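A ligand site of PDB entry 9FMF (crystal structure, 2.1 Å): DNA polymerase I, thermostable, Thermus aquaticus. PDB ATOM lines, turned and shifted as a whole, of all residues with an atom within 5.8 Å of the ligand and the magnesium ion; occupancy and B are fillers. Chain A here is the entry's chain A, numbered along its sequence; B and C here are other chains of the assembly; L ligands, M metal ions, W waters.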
ATOM      1  N   ARG A 281      -2.760  22.895   8.767  1.00  0.00           N
ATOM      2  CA  ARG A 281      -3.477  21.635   8.798  1.00  0.00           C
ATOM      3  C   ARG A 281      -4.954  21.837   8.444  1.00  0.00           C
ATOM      4  O   ARG A 281      -5.520  22.929   8.626  1.00  0.00           O
ATOM      5  CB  ARG A 281      -3.373  20.984  10.170  1.00  0.00           C
ATOM      6  CG  ARG A 281      -2.075  20.346  10.490  1.00  0.00           C
ATOM      7  CD  ARG A 281      -2.284  19.560  11.765  1.00  0.00           C
ATOM      8  NE  ARG A 281      -1.172  18.688  12.070  1.00  0.00           N
ATOM      9  CZ  ARG A 281      -1.188  17.761  13.019  1.00  0.00           C
ATOM     10  NH1 ARG A 281      -2.255  17.597  13.790  1.00  0.00           N
ATOM     11  NH2 ARG A 281      -0.136  16.972  13.185  1.00  0.00           N
ATOM     12  N   VAL A 294      -8.129   4.754  18.712  1.00  0.00           N
ATOM     13  CA  VAL A 294      -7.340   3.672  18.127  1.00  0.00           C
ATOM     14  C   VAL A 294      -6.413   3.033  19.152  1.00  0.00           C
ATOM     15  O   VAL A 294      -6.064   1.852  19.030  1.00  0.00           O
ATOM     16  CB  VAL A 294      -6.573   4.186  16.911  1.00  0.00           C
ATOM     17  CG1 VAL A 294      -5.548   5.228  17.330  1.00  0.00           C
ATOM     18  CG2 VAL A 294      -5.918   3.023  16.172  1.00  0.00           C
ATOM     19  N   ARG A 295      -6.003   3.794  20.171  1.00  0.00           N
ATOM     20  CA  ARG A 295      -4.880   3.363  20.996  1.00  0.00           C
ATOM     21  C   ARG A 295      -5.261   2.273  21.985  1.00  0.00           C
ATOM     22  O   ARG A 295      -4.506   1.317  22.174  1.00  0.00           O
ATOM     23  CB  ARG A 295      -4.293   4.579  21.713  1.00  0.00           C
ATOM     24  CG  ARG A 295      -3.824   5.643  20.735  1.00  0.00           C
ATOM     25  CD  ARG A 295      -3.134   6.793  21.436  1.00  0.00           C
ATOM     26  NE  ARG A 295      -2.047   6.306  22.270  1.00  0.00           N
ATOM     27  CZ  ARG A 295      -1.159   7.071  22.873  1.00  0.00           C
ATOM     28  NH1 ARG A 295      -1.195   8.392  22.780  1.00  0.00           N
ATOM     29  NH2 ARG A 295      -0.174   6.495  23.577  1.00  0.00           N
ATOM     30  N   ASP A 318      -0.100   6.314   5.248  1.00  0.00           N
ATOM     31  CA  ASP A 318       0.345   7.046   6.428  1.00  0.00           C
ATOM     32  C   ASP A 318       1.840   7.324   6.254  1.00  0.00           C
ATOM     33  O   ASP A 318       2.616   6.367   6.113  1.00  0.00           O
ATOM     34  CB  ASP A 318       0.077   6.195   7.694  1.00  0.00           C
ATOM     35  CG  ASP A 318       0.368   6.945   9.045  1.00  0.00           C
ATOM     36  OD1 ASP A 318       1.169   7.914   9.091  1.00  0.00           O
ATOM     37  OD2 ASP A 318      -0.218   6.529  10.090  1.00  0.00           O
ATOM     38  N   TYR A 319       2.233   8.598   6.210  1.00  0.00           N
ATOM     39  CA  TYR A 319       3.641   8.968   6.160  1.00  0.00           C
ATOM     40  C   TYR A 319       4.342   8.550   7.449  1.00  0.00           C
ATOM     41  O   TYR A 319       3.819   8.767   8.551  1.00  0.00           O
ATOM     42  CB  TYR A 319       3.819  10.474   5.972  1.00  0.00           C
ATOM     43  CG  TYR A 319       3.537  10.982   4.584  1.00  0.00           C
ATOM     44  CD1 TYR A 319       4.368  10.666   3.526  1.00  0.00           C
ATOM     45  CD2 TYR A 319       2.442  11.803   4.341  1.00  0.00           C
ATOM     46  CE1 TYR A 319       4.111  11.137   2.228  1.00  0.00           C
ATOM     47  CE2 TYR A 319       2.171  12.284   3.060  1.00  0.00           C
ATOM     48  CZ  TYR A 319       3.012  11.954   2.018  1.00  0.00           C
ATOM     49  OH  TYR A 319       2.732  12.438   0.757  1.00  0.00           O
ATOM     50  N   SER A 320       5.551   8.002   7.307  1.00  0.00           N
ATOM     51  CA  SER A 320       6.316   7.576   8.473  1.00  0.00           C
ATOM     52  C   SER A 320       7.168   8.716   9.011  1.00  0.00           C
ATOM     53  O   SER A 320       7.834   9.411   8.238  1.00  0.00           O
ATOM     54  CB  SER A 320       7.233   6.405   8.126  1.00  0.00           C
ATOM     55  OG  SER A 320       8.552   6.876   7.963  1.00  0.00           O
ATOM     56  N   GLN A 321       7.164   8.889  10.344  1.00  0.00           N
ATOM     57  CA  GLN A 321       8.030   9.848  11.034  1.00  0.00           C
ATOM     58  C   GLN A 321       8.076  11.185  10.298  1.00  0.00           C
ATOM     59  O   GLN A 321       9.129  11.742  10.022  1.00  0.00           O
ATOM     60  CB  GLN A 321       9.437   9.300  11.216  1.00  0.00           C
ATOM     61  CG  GLN A 321       9.532   7.862  11.716  1.00  0.00           C
ATOM     62  CD  GLN A 321      10.968   7.349  11.779  1.00  0.00           C
ATOM     63  OE1 GLN A 321      11.738   7.717  12.674  1.00  0.00           O
ATOM     64  NE2 GLN A 321      11.332   6.492  10.824  1.00  0.00           N
ATOM     65  N   ILE A 322       6.887  11.688   9.967  1.00  0.00           N
ATOM     66  CA  ILE A 322       6.794  12.699   8.932  1.00  0.00           C
ATOM     67  C   ILE A 322       7.441  14.011   9.381  1.00  0.00           C
ATOM     68  O   ILE A 322       8.273  14.577   8.680  1.00  0.00           O
ATOM     69  CB  ILE A 322       5.331  12.883   8.478  1.00  0.00           C
ATOM     70  CG1 ILE A 322       5.218  14.053   7.501  1.00  0.00           C
ATOM     71  CG2 ILE A 322       4.406  13.016   9.665  1.00  0.00           C
ATOM     72  CD1 ILE A 322       5.726  13.720   6.089  1.00  0.00           C
ATOM     73  N   GLU A 323       7.087  14.496  10.579  1.00  0.00           N
ATOM     74  CA  GLU A 323       7.655  15.779  11.016  1.00  0.00           C
ATOM     75  C   GLU A 323       9.142  15.691  11.328  1.00  0.00           C
ATOM     76  O   GLU A 323       9.826  16.725  11.315  1.00  0.00           O
ATOM     77  CB  GLU A 323       6.857  16.330  12.211  1.00  0.00           C
ATOM     78  CG  GLU A 323       5.428  16.795  11.783  1.00  0.00           C
ATOM     79  CD  GLU A 323       4.578  17.431  12.893  1.00  0.00           C
ATOM     80  OE1 GLU A 323       5.128  17.991  13.872  1.00  0.00           O
ATOM     81  OE2 GLU A 323       3.324  17.353  12.775  1.00  0.00           O
ATOM     82  N   LEU A 324       9.704  14.490  11.549  1.00  0.00           N
ATOM     83  CA  LEU A 324      11.142  14.384  11.729  1.00  0.00           C
ATOM     84  C   LEU A 324      11.884  14.489  10.396  1.00  0.00           C
ATOM     85  O   LEU A 324      12.931  15.143  10.319  1.00  0.00           O
ATOM     86  CB  LEU A 324      11.507  13.073  12.444  1.00  0.00           C
ATOM     87  CG  LEU A 324      11.001  12.933  13.880  1.00  0.00           C
ATOM     88  CD1 LEU A 324      11.179  11.526  14.424  1.00  0.00           C
ATOM     89  CD2 LEU A 324      11.744  13.923  14.759  1.00  0.00           C
ATOM     90  N   HIS A 347      11.290   6.424  16.551  1.00  0.00           N
ATOM     91  CA  HIS A 347      10.315   6.052  17.571  1.00  0.00           C
ATOM     92  C   HIS A 347      10.582   4.662  18.142  1.00  0.00           C
ATOM     93  O   HIS A 347      10.371   4.452  19.334  1.00  0.00           O
ATOM     94  CB  HIS A 347       8.882   6.130  17.018  1.00  0.00           C
ATOM     95  CG  HIS A 347       8.539   7.456  16.404  1.00  0.00           C
ATOM     96  ND1 HIS A 347       9.087   8.644  16.822  1.00  0.00           N
ATOM     97  CD2 HIS A 347       7.697   7.776  15.382  1.00  0.00           C
ATOM     98  CE1 HIS A 347       8.597   9.638  16.103  1.00  0.00           C
ATOM     99  NE2 HIS A 347       7.752   9.137  15.212  1.00  0.00           N
ATOM    100  N   ARG A 367       5.900   1.649  21.018  1.00  0.00           N
ATOM    101  CA  ARG A 367       6.261   2.649  20.019  1.00  0.00           C
ATOM    102  C   ARG A 367       5.370   3.882  20.130  1.00  0.00           C
ATOM    103  O   ARG A 367       5.841   5.008  19.993  1.00  0.00           O
ATOM    104  CB  ARG A 367       6.175   2.035  18.622  1.00  0.00           C
ATOM    105  CG  ARG A 367       6.963   2.763  17.542  1.00  0.00           C
ATOM    106  CD  ARG A 367       6.805   2.098  16.163  1.00  0.00           C
ATOM    107  NE  ARG A 367       7.380   2.927  15.114  1.00  0.00           N
ATOM    108  CZ  ARG A 367       6.726   3.890  14.488  1.00  0.00           C
ATOM    109  NH1 ARG A 367       5.438   4.108  14.708  1.00  0.00           N
ATOM    110  NH2 ARG A 367       7.377   4.664  13.621  1.00  0.00           N
ATOM    111  N   ARG A 368       4.077   3.669  20.401  1.00  0.00           N
ATOM    112  CA  ARG A 368       3.159   4.789  20.586  1.00  0.00           C
ATOM    113  C   ARG A 368       3.618   5.688  21.725  1.00  0.00           C
ATOM    114  O   ARG A 368       3.499   6.915  21.654  1.00  0.00           O
ATOM    115  CB  ARG A 368       1.739   4.280  20.846  1.00  0.00           C
ATOM    116  CG  ARG A 368       1.097   3.499  19.701  1.00  0.00           C
ATOM    117  CD  ARG A 368      -0.320   3.068  20.093  1.00  0.00           C
ATOM    118  NE  ARG A 368      -0.940   2.114  19.172  1.00  0.00           N
ATOM    119  CZ  ARG A 368      -1.400   2.417  17.962  1.00  0.00           C
ATOM    120  NH1 ARG A 368      -1.235   3.605  17.422  1.00  0.00           N
ATOM    121  NH2 ARG A 368      -2.034   1.475  17.260  1.00  0.00           N
ATOM    122  N   ALA A 369       4.134   5.095  22.798  1.00  0.00           N
ATOM    123  CA  ALA A 369       4.600   5.894  23.922  1.00  0.00           C
ATOM    124  C   ALA A 369       5.817   6.724  23.538  1.00  0.00           C
ATOM    125  O   ALA A 369       5.936   7.898  23.908  1.00  0.00           O
ATOM    126  CB  ALA A 369       4.920   4.984  25.107  1.00  0.00           C
ATOM    127  N   LYS A 371       6.480   7.811  20.585  1.00  0.00           N
ATOM    128  CA  LYS A 371       6.082   8.890  19.677  1.00  0.00           C
ATOM    129  C   LYS A 371       5.752  10.151  20.463  1.00  0.00           C
ATOM    130  O   LYS A 371       6.284  11.228  20.196  1.00  0.00           O
ATOM    131  CB  LYS A 371       4.896   8.449  18.820  1.00  0.00           C
ATOM    132  CG  LYS A 371       5.307   7.550  17.679  1.00  0.00           C
ATOM    133  CD  LYS A 371       4.143   6.750  17.115  1.00  0.00           C
ATOM    134  CE  LYS A 371       3.146   7.637  16.466  1.00  0.00           C
ATOM    135  NZ  LYS A 371       3.519   7.812  15.046  1.00  0.00           N
ATOM    136  N   THR A 372       4.880  10.028  21.478  1.00  0.00           N
ATOM    137  CA  THR A 372       4.538  11.207  22.262  1.00  0.00           C
ATOM    138  C   THR A 372       5.753  11.748  23.008  1.00  0.00           C
ATOM    139  O   THR A 372       5.890  12.965  23.171  1.00  0.00           O
ATOM    140  CB  THR A 372       3.395  10.868  23.223  1.00  0.00           C
ATOM    141  OG1 THR A 372       3.928  10.544  24.517  1.00  0.00           O
ATOM    142  CG2 THR A 372       2.580   9.708  22.704  1.00  0.00           C
ATOM    143  N   PHE A 375       8.118  13.618  20.275  1.00  0.00           N
ATOM    144  CA  PHE A 375       7.541  14.888  19.868  1.00  0.00           C
ATOM    145  C   PHE A 375       7.366  15.817  21.057  1.00  0.00           C
ATOM    146  O   PHE A 375       7.453  17.040  20.896  1.00  0.00           O
ATOM    147  CB  PHE A 375       6.221  14.643  19.128  1.00  0.00           C
ATOM    148  CG  PHE A 375       6.419  14.010  17.767  1.00  0.00           C
ATOM    149  CD1 PHE A 375       7.323  14.566  16.859  1.00  0.00           C
ATOM    150  CD2 PHE A 375       5.777  12.826  17.420  1.00  0.00           C
ATOM    151  CE1 PHE A 375       7.553  14.005  15.632  1.00  0.00           C
ATOM    152  CE2 PHE A 375       6.017  12.238  16.172  1.00  0.00           C
ATOM    153  CZ  PHE A 375       6.900  12.841  15.288  1.00  0.00           C
ATOM    154  N   GLY A 376       7.171  15.268  22.246  1.00  0.00           N
ATOM    155  CA  GLY A 376       7.191  16.096  23.434  1.00  0.00           C
ATOM    156  C   GLY A 376       8.519  16.793  23.624  1.00  0.00           C
ATOM    157  O   GLY A 376       8.571  18.013  23.773  1.00  0.00           O
ATOM    158  N   TYR A 379       9.504  19.578  20.778  1.00  0.00           N
ATOM    159  CA  TYR A 379       8.855  20.878  20.763  1.00  0.00           C
ATOM    160  C   TYR A 379       8.967  21.622  22.069  1.00  0.00           C
ATOM    161  O   TYR A 379       8.281  22.633  22.235  1.00  0.00           O
ATOM    162  CB  TYR A 379       7.386  20.721  20.370  1.00  0.00           C
ATOM    163  CG  TYR A 379       7.273  20.292  18.948  1.00  0.00           C
ATOM    164  CD1 TYR A 379       7.811  21.075  17.937  1.00  0.00           C
ATOM    165  CD2 TYR A 379       6.658  19.106  18.614  1.00  0.00           C
ATOM    166  CE1 TYR A 379       7.737  20.674  16.623  1.00  0.00           C
ATOM    167  CE2 TYR A 379       6.562  18.707  17.309  1.00  0.00           C
ATOM    168  CZ  TYR A 379       7.108  19.502  16.315  1.00  0.00           C
ATOM    169  OH  TYR A 379       7.008  19.090  15.015  1.00  0.00           O
ATOM    170  N   ASN A 458       7.317  25.467  15.977  1.00  0.00           N
ATOM    171  CA  ASN A 458       6.567  24.278  15.598  1.00  0.00           C
ATOM    172  C   ASN A 458       5.873  24.458  14.258  1.00  0.00           C
ATOM    173  O   ASN A 458       5.781  23.516  13.473  1.00  0.00           O
ATOM    174  CB  ASN A 458       5.536  23.936  16.659  1.00  0.00           C
ATOM    175  CG  ASN A 458       4.509  22.974  16.158  1.00  0.00           C
ATOM    176  OD1 ASN A 458       3.409  23.367  15.784  1.00  0.00           O
ATOM    177  ND2 ASN A 458       4.865  21.702  16.112  1.00  0.00           N
ATOM    178  N   GLN A 462       5.275  21.606  11.265  1.00  0.00           N
ATOM    179  CA  GLN A 462       3.977  20.946  11.157  1.00  0.00           C
ATOM    180  C   GLN A 462       3.207  21.449   9.942  1.00  0.00           C
ATOM    181  O   GLN A 462       2.458  20.681   9.332  1.00  0.00           O
ATOM    182  CB  GLN A 462       3.181  21.151  12.449  1.00  0.00           C
ATOM    183  CG  GLN A 462       1.739  20.690  12.350  1.00  0.00           C
ATOM    184  CD  GLN A 462       0.881  21.190  13.510  1.00  0.00           C
ATOM    185  OE1 GLN A 462      -0.095  21.917  13.315  1.00  0.00           O
ATOM    186  NE2 GLN A 462       1.233  20.773  14.727  1.00  0.00           N
ATOM    187  N   ASP A 493      -1.541  13.235   8.399  1.00  0.00           N
ATOM    188  CA  ASP A 493      -0.457  12.660   7.613  1.00  0.00           C
ATOM    189  C   ASP A 493      -0.895  11.360   6.952  1.00  0.00           C
ATOM    190  O   ASP A 493      -0.063  10.618   6.435  1.00  0.00           O
ATOM    191  CB  ASP A 493       0.806  12.463   8.462  1.00  0.00           C
ATOM    192  CG  ASP A 493       0.714  11.274   9.399  1.00  0.00           C
ATOM    193  OD1 ASP A 493      -0.368  11.061  10.006  1.00  0.00           O
ATOM    194  OD2 ASP A 493       1.726  10.545   9.531  1.00  0.00           O
ATOM    195  P    DA B   4       5.792  21.535  29.392  1.00  0.00           P
ATOM    196  OP1  DA B   4       4.514  20.989  29.872  1.00  0.00           O
ATOM    197  OP2  DA B   4       7.050  21.145  30.066  1.00  0.00           O
ATOM    198  O5'  DA B   4       5.921  21.173  27.844  1.00  0.00           O
ATOM    199  C5'  DA B   4       4.943  21.648  26.932  1.00  0.00           C
ATOM    200  C4'  DA B   4       5.524  21.754  25.542  1.00  0.00           C
ATOM    201  O4'  DA B   4       6.067  20.470  25.154  1.00  0.00           O
ATOM    202  C3'  DA B   4       4.519  22.100  24.464  1.00  0.00           C
ATOM    203  O3'  DA B   4       4.440  23.506  24.339  1.00  0.00           O
ATOM    204  C2'  DA B   4       5.126  21.460  23.222  1.00  0.00           C
ATOM    205  C1'  DA B   4       5.756  20.190  23.800  1.00  0.00           C
ATOM    206  N9   DA B   4       4.909  18.999  23.771  1.00  0.00           N
ATOM    207  C8   DA B   4       4.406  18.300  24.848  1.00  0.00           C
ATOM    208  N7   DA B   4       3.677  17.257  24.522  1.00  0.00           N
ATOM    209  C5   DA B   4       3.694  17.273  23.142  1.00  0.00           C
ATOM    210  C6   DA B   4       3.130  16.415  22.187  1.00  0.00           C
ATOM    211  N6   DA B   4       2.391  15.352  22.507  1.00  0.00           N
ATOM    212  N1   DA B   4       3.348  16.695  20.873  1.00  0.00           N
ATOM    213  C2   DA B   4       4.087  17.758  20.553  1.00  0.00           C
ATOM    214  N3   DA B   4       4.681  18.641  21.361  1.00  0.00           N
ATOM    215  C4   DA B   4       4.451  18.336  22.662  1.00  0.00           C
ATOM    216  P    DG B   5       3.013  24.212  24.151  1.00  0.00           P
ATOM    217  OP1  DG B   5       3.210  25.662  24.400  1.00  0.00           O
ATOM    218  OP2  DG B   5       1.991  23.475  24.942  1.00  0.00           O
ATOM    219  O5'  DG B   5       2.641  23.961  22.615  1.00  0.00           O
ATOM    220  C5'  DG B   5       3.414  24.524  21.583  1.00  0.00           C
ATOM    221  C4'  DG B   5       3.083  23.886  20.233  1.00  0.00           C
ATOM    222  O4'  DG B   5       3.368  22.473  20.259  1.00  0.00           O
ATOM    223  C3'  DG B   5       1.634  23.951  19.802  1.00  0.00           C
ATOM    224  O3'  DG B   5       1.334  25.235  19.237  1.00  0.00           O
ATOM    225  C2'  DG B   5       1.602  22.855  18.745  1.00  0.00           C
ATOM    226  C1'  DG B   5       2.534  21.812  19.321  1.00  0.00           C
ATOM    227  N9   DG B   5       1.831  20.767  20.020  1.00  0.00           N
ATOM    228  C8   DG B   5       1.687  20.633  21.366  1.00  0.00           C
ATOM    229  N7   DG B   5       0.978  19.587  21.714  1.00  0.00           N
ATOM    230  C5   DG B   5       0.663  18.990  20.509  1.00  0.00           C
ATOM    231  C6   DG B   5      -0.072  17.790  20.240  1.00  0.00           C
ATOM    232  O6   DG B   5      -0.606  17.020  21.055  1.00  0.00           O
ATOM    233  N1   DG B   5      -0.189  17.554  18.875  1.00  0.00           N
ATOM    234  C2   DG B   5       0.358  18.331  17.898  1.00  0.00           C
ATOM    235  N2   DG B   5       0.146  17.925  16.635  1.00  0.00           N
ATOM    236  N3   DG B   5       1.074  19.429  18.129  1.00  0.00           N
ATOM    237  C4   DG B   5       1.166  19.699  19.460  1.00  0.00           C
ATOM    238  P    DA C  11      -6.853   7.996  20.959  1.00  0.00           P
ATOM    239  OP1  DA C  11      -6.916   6.601  20.469  1.00  0.00           O
ATOM    240  OP2  DA C  11      -5.905   8.387  22.010  1.00  0.00           O
ATOM    241  O5'  DA C  11      -6.557   8.891  19.666  1.00  0.00           O
ATOM    242  C5'  DA C  11      -7.454   8.797  18.592  1.00  0.00           C
ATOM    243  C4'  DA C  11      -7.192   9.857  17.558  1.00  0.00           C
ATOM    244  O4'  DA C  11      -7.464  11.163  18.104  1.00  0.00           O
ATOM    245  C3'  DA C  11      -5.775   9.888  17.026  1.00  0.00           C
ATOM    246  O3'  DA C  11      -5.728   9.119  15.818  1.00  0.00           O
ATOM    247  C2'  DA C  11      -5.531  11.365  16.722  1.00  0.00           C
ATOM    248  C1'  DA C  11      -6.569  12.108  17.575  1.00  0.00           C
ATOM    249  N9   DA C  11      -5.965  12.857  18.667  1.00  0.00           N
ATOM    250  C8   DA C  11      -5.633  12.406  19.928  1.00  0.00           C
ATOM    251  N7   DA C  11      -5.060  13.327  20.679  1.00  0.00           N
ATOM    252  C5   DA C  11      -5.035  14.447  19.862  1.00  0.00           C
ATOM    253  C6   DA C  11      -4.582  15.771  20.046  1.00  0.00           C
ATOM    254  N6   DA C  11      -4.031  16.193  21.183  1.00  0.00           N
ATOM    255  N1   DA C  11      -4.710  16.639  19.020  1.00  0.00           N
ATOM    256  C2   DA C  11      -5.274  16.216  17.872  1.00  0.00           C
ATOM    257  N3   DA C  11      -5.731  15.006  17.572  1.00  0.00           N
ATOM    258  C4   DA C  11      -5.592  14.166  18.620  1.00  0.00           C
ATOM    259  N1  DOC C  12      -2.148  13.809  16.243  1.00  0.00           N
ATOM    260  C2  DOC C  12      -1.541  15.007  16.754  1.00  0.00           C
ATOM    261  N3  DOC C  12      -1.247  15.075  18.132  1.00  0.00           N
ATOM    262  C4  DOC C  12      -1.573  14.031  18.925  1.00  0.00           C
ATOM    263  C5  DOC C  12      -2.183  12.819  18.418  1.00  0.00           C
ATOM    264  C6  DOC C  12      -2.443  12.767  17.088  1.00  0.00           C
ATOM    265  O2  DOC C  12      -1.294  15.910  15.979  1.00  0.00           O
ATOM    266  N4  DOC C  12      -1.288  14.162  20.258  1.00  0.00           N
ATOM    267  C1' DOC C  12      -2.463  13.654  14.800  1.00  0.00           C
ATOM    268  C2' DOC C  12      -1.204  13.249  13.977  1.00  0.00           C
ATOM    269  C3' DOC C  12      -1.453  11.774  13.683  1.00  0.00           C
ATOM    270  C4' DOC C  12      -2.956  11.783  13.548  1.00  0.00           C
ATOM    271  O4' DOC C  12      -3.410  12.648  14.605  1.00  0.00           O
ATOM    272  C5' DOC C  12      -3.600  10.444  13.802  1.00  0.00           C
ATOM    273  O5' DOC C  12      -3.268   9.997  15.073  1.00  0.00           O
ATOM    274  P   DOC C  12      -4.173   8.815  15.711  1.00  0.00           P
ATOM    275  OP1 DOC C  12      -4.447   7.789  14.685  1.00  0.00           O
ATOM    276  OP2 DOC C  12      -3.444   8.263  16.997  1.00  0.00           O
HETATM  277  C1  LIG L   1       2.644  13.701  13.112  1.00  0.00           C
HETATM  278  C2  LIG L   1       2.001  12.453  12.566  1.00  0.00           C
HETATM  279  C3  LIG L   1       2.183  13.741  19.099  1.00  0.00           C
HETATM  280  C4  LIG L   1       2.006  13.305  16.729  1.00  0.00           C
HETATM  281  C5  LIG L   1       1.885  12.841  18.016  1.00  0.00           C
HETATM  282  C6  LIG L   1       1.465  11.464  18.290  1.00  0.00           C
HETATM  283  C7  LIG L   1       1.655  10.663  19.356  1.00  0.00           C
HETATM  284  C8  LIG L   1       0.957   9.434  19.078  1.00  0.00           C
HETATM  285  C9  LIG L   1       0.668   8.244  19.755  1.00  0.00           C
HETATM  286  C10 LIG L   1      -0.161   7.331  19.155  1.00  0.00           C
HETATM  287  C11 LIG L   1      -0.720   7.510  17.914  1.00  0.00           C
HETATM  288  C12 LIG L   1      -0.442   8.675  17.225  1.00  0.00           C
HETATM  289  C13 LIG L   1       0.390   9.601  17.820  1.00  0.00           C
HETATM  290  C14 LIG L   1       2.735  15.488  17.434  1.00  0.00           C
HETATM  291  C15 LIG L   1       2.677  15.018  15.037  1.00  0.00           C
HETATM  292  C16 LIG L   1       4.123  14.774  14.586  1.00  0.00           C
HETATM  293  C17 LIG L   1       4.010  13.501  13.751  1.00  0.00           C
HETATM  294  F1  LIG L   1      -0.482   6.200  19.842  1.00  0.00           F
HETATM  295  N1  LIG L   1       2.598  15.011  18.715  1.00  0.00           N
HETATM  296  N2  LIG L   1       2.434  14.582  16.439  1.00  0.00           N
HETATM  297  O1  LIG L   1       2.094  13.458  20.288  1.00  0.00           O
HETATM  298  O2  LIG L   1       5.069  13.391  12.794  1.00  0.00           O
HETATM  299  O3  LIG L   1       1.662  11.592  13.663  1.00  0.00           O
HETATM  300  O4  LIG L   1       1.580   9.677  12.107  1.00  0.00           O
HETATM  301  O5  LIG L   1       1.212   9.275  14.581  1.00  0.00           O
HETATM  302  O6  LIG L   1       3.476  10.055  13.739  1.00  0.00           O
HETATM  303  O7  LIG L   1       4.252  10.032  11.368  1.00  0.00           O
HETATM  304  O8  LIG L   1       5.898  10.595  13.214  1.00  0.00           O
HETATM  305  O9  LIG L   1       4.898   8.263  13.047  1.00  0.00           O
HETATM  306  O10 LIG L   1       5.840   6.516  11.709  1.00  0.00           O
HETATM  307  O11 LIG L   1       4.055   5.779  13.335  1.00  0.00           O
HETATM  308  O12 LIG L   1       3.441   7.202  11.346  1.00  0.00           O
HETATM  309  O13 LIG L   1       1.841  14.261  14.177  1.00  0.00           O
HETATM  310  O14 LIG L   1       0.695  10.846  17.326  1.00  0.00           O
HETATM  311  O15 LIG L   1       3.137  16.623  17.207  1.00  0.00           O
HETATM  312  P1  LIG L   1       1.890  10.035  13.507  1.00  0.00           P
HETATM  313  P2  LIG L   1       4.714   9.824  12.756  1.00  0.00           P
HETATM  314  P3  LIG L   1       4.514   6.838  12.359  1.00  0.00           P
HETATM  315 MG    MG M   1       2.829   8.941  10.276  1.00  0.00          MG
HETATM  316  O   HOH W   1      -0.606   7.935  13.358  1.00  0.00           O
HETATM  317  O   HOH W   2       1.398   5.962  12.309  1.00  0.00           O
HETATM  318  O   HOH W   3      -1.414   9.052  11.084  1.00  0.00           O
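N of Gln 321 sits at hydrogen-bond distance from O10 of the ligand.
The side-chain amino group (NZ) of Lys 371 lies within salt-bridge range of an oxygen (O11) of the ligand, 2.7 Å away.
N of Glu 323 sits at hydrogen-bond distance from O2 of the ligand.
N1 of DA 4 of chain B lies within hydrogen-bond range of a nitrogen (N1) of the ligand.
An oxygen (O7) of the ligand lies close to the backbone NH (N) of Ile 322, at 3.4 Å.
O13 of the ligand is in hydrogen-bond range of NH2 of Arg 281 (3.5 Å).
An oxygen (O11) of the ligand is in salt-bridge range of the guanidinium group of Arg 367 (2.6 Å).
An oxygen (O8) of the ligand is in hydrogen-bond range of a ring nitrogen (NE2) of His 347 (3.1 Å).
The guanidinium group (NE) of Arg 295 sits close to a fluorine (F1) of the ligand (2.9 Å).
An oxygen (O15) of the ligand sits close to N2 of DG 5 of chain B, 3.3 Å away.
N4 of DOC 12 of chain C lies close to O1 of the ligand, at 3.5 Å.
Ser 320 touches the ligand.
Arg 368 touches the ligand (CB to F1, 3.1 Å).
Thr 372 touches the ligand (CG2 to C7, 3.6 Å).
Phe 375 touches the ligand.
Hydrophobic or aromatic side chains that line the ligand: Ile 322, His 347 and Phe 375.
Of the 26 residues printed, 3 come within 4 Å of the magnesium ion.
Along chain A the residues within 4 Å of the magnesium ion span positions 318 to 493.
Water W2 lies within hydrogen-bond range of OD2 of Asp 318 (2.8 Å) and O11 of the ligand (2.9 Å).
Water W3 lies within hydrogen-bond range of OD1 of Asp 493 and OD2 of Asp 318.
The magnesium ion is bound by O of Tyr 319 (2.0 Å), OD2 of Asp 493 (2.1 Å), O7 of the ligand (2.1 Å), O12 of the ligand (2.1 Å), OD1 of Asp 318 (2.3 Å) and O4 of the ligand (2.3 Å).
The magnesium ion has six donor atoms within binding distance.
O2 of DOC 12 of chain C lies within hydrogen-bond range of the guanidinium group (NH1) of Arg 281, at 2.9 Å.
N of Arg 295 sits at hydrogen-bond distance from OP1 of DA 11 of chain C (3.0 Å).
The side-chain hydroxyl (OG1) of Thr 372 sits at hydrogen-bond distance from the backbone carbonyl oxygen (O) of Ala 369 (3.4 Å).
The side-chain carboxylate (OE2) of Glu 323 is in salt-bridge range of the guanidinium group (NH2) of Arg 281, 3.5 Å away.
O2 of DOC 12 of chain C sits close to N2 of DG 5 of chain B (2.6 Å).
The side-chain carboxylate (OE1) of Glu 323 sits at hydrogen-bond distance from the side-chain hydroxyl (OH) of Tyr 379 (2.5 Å).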
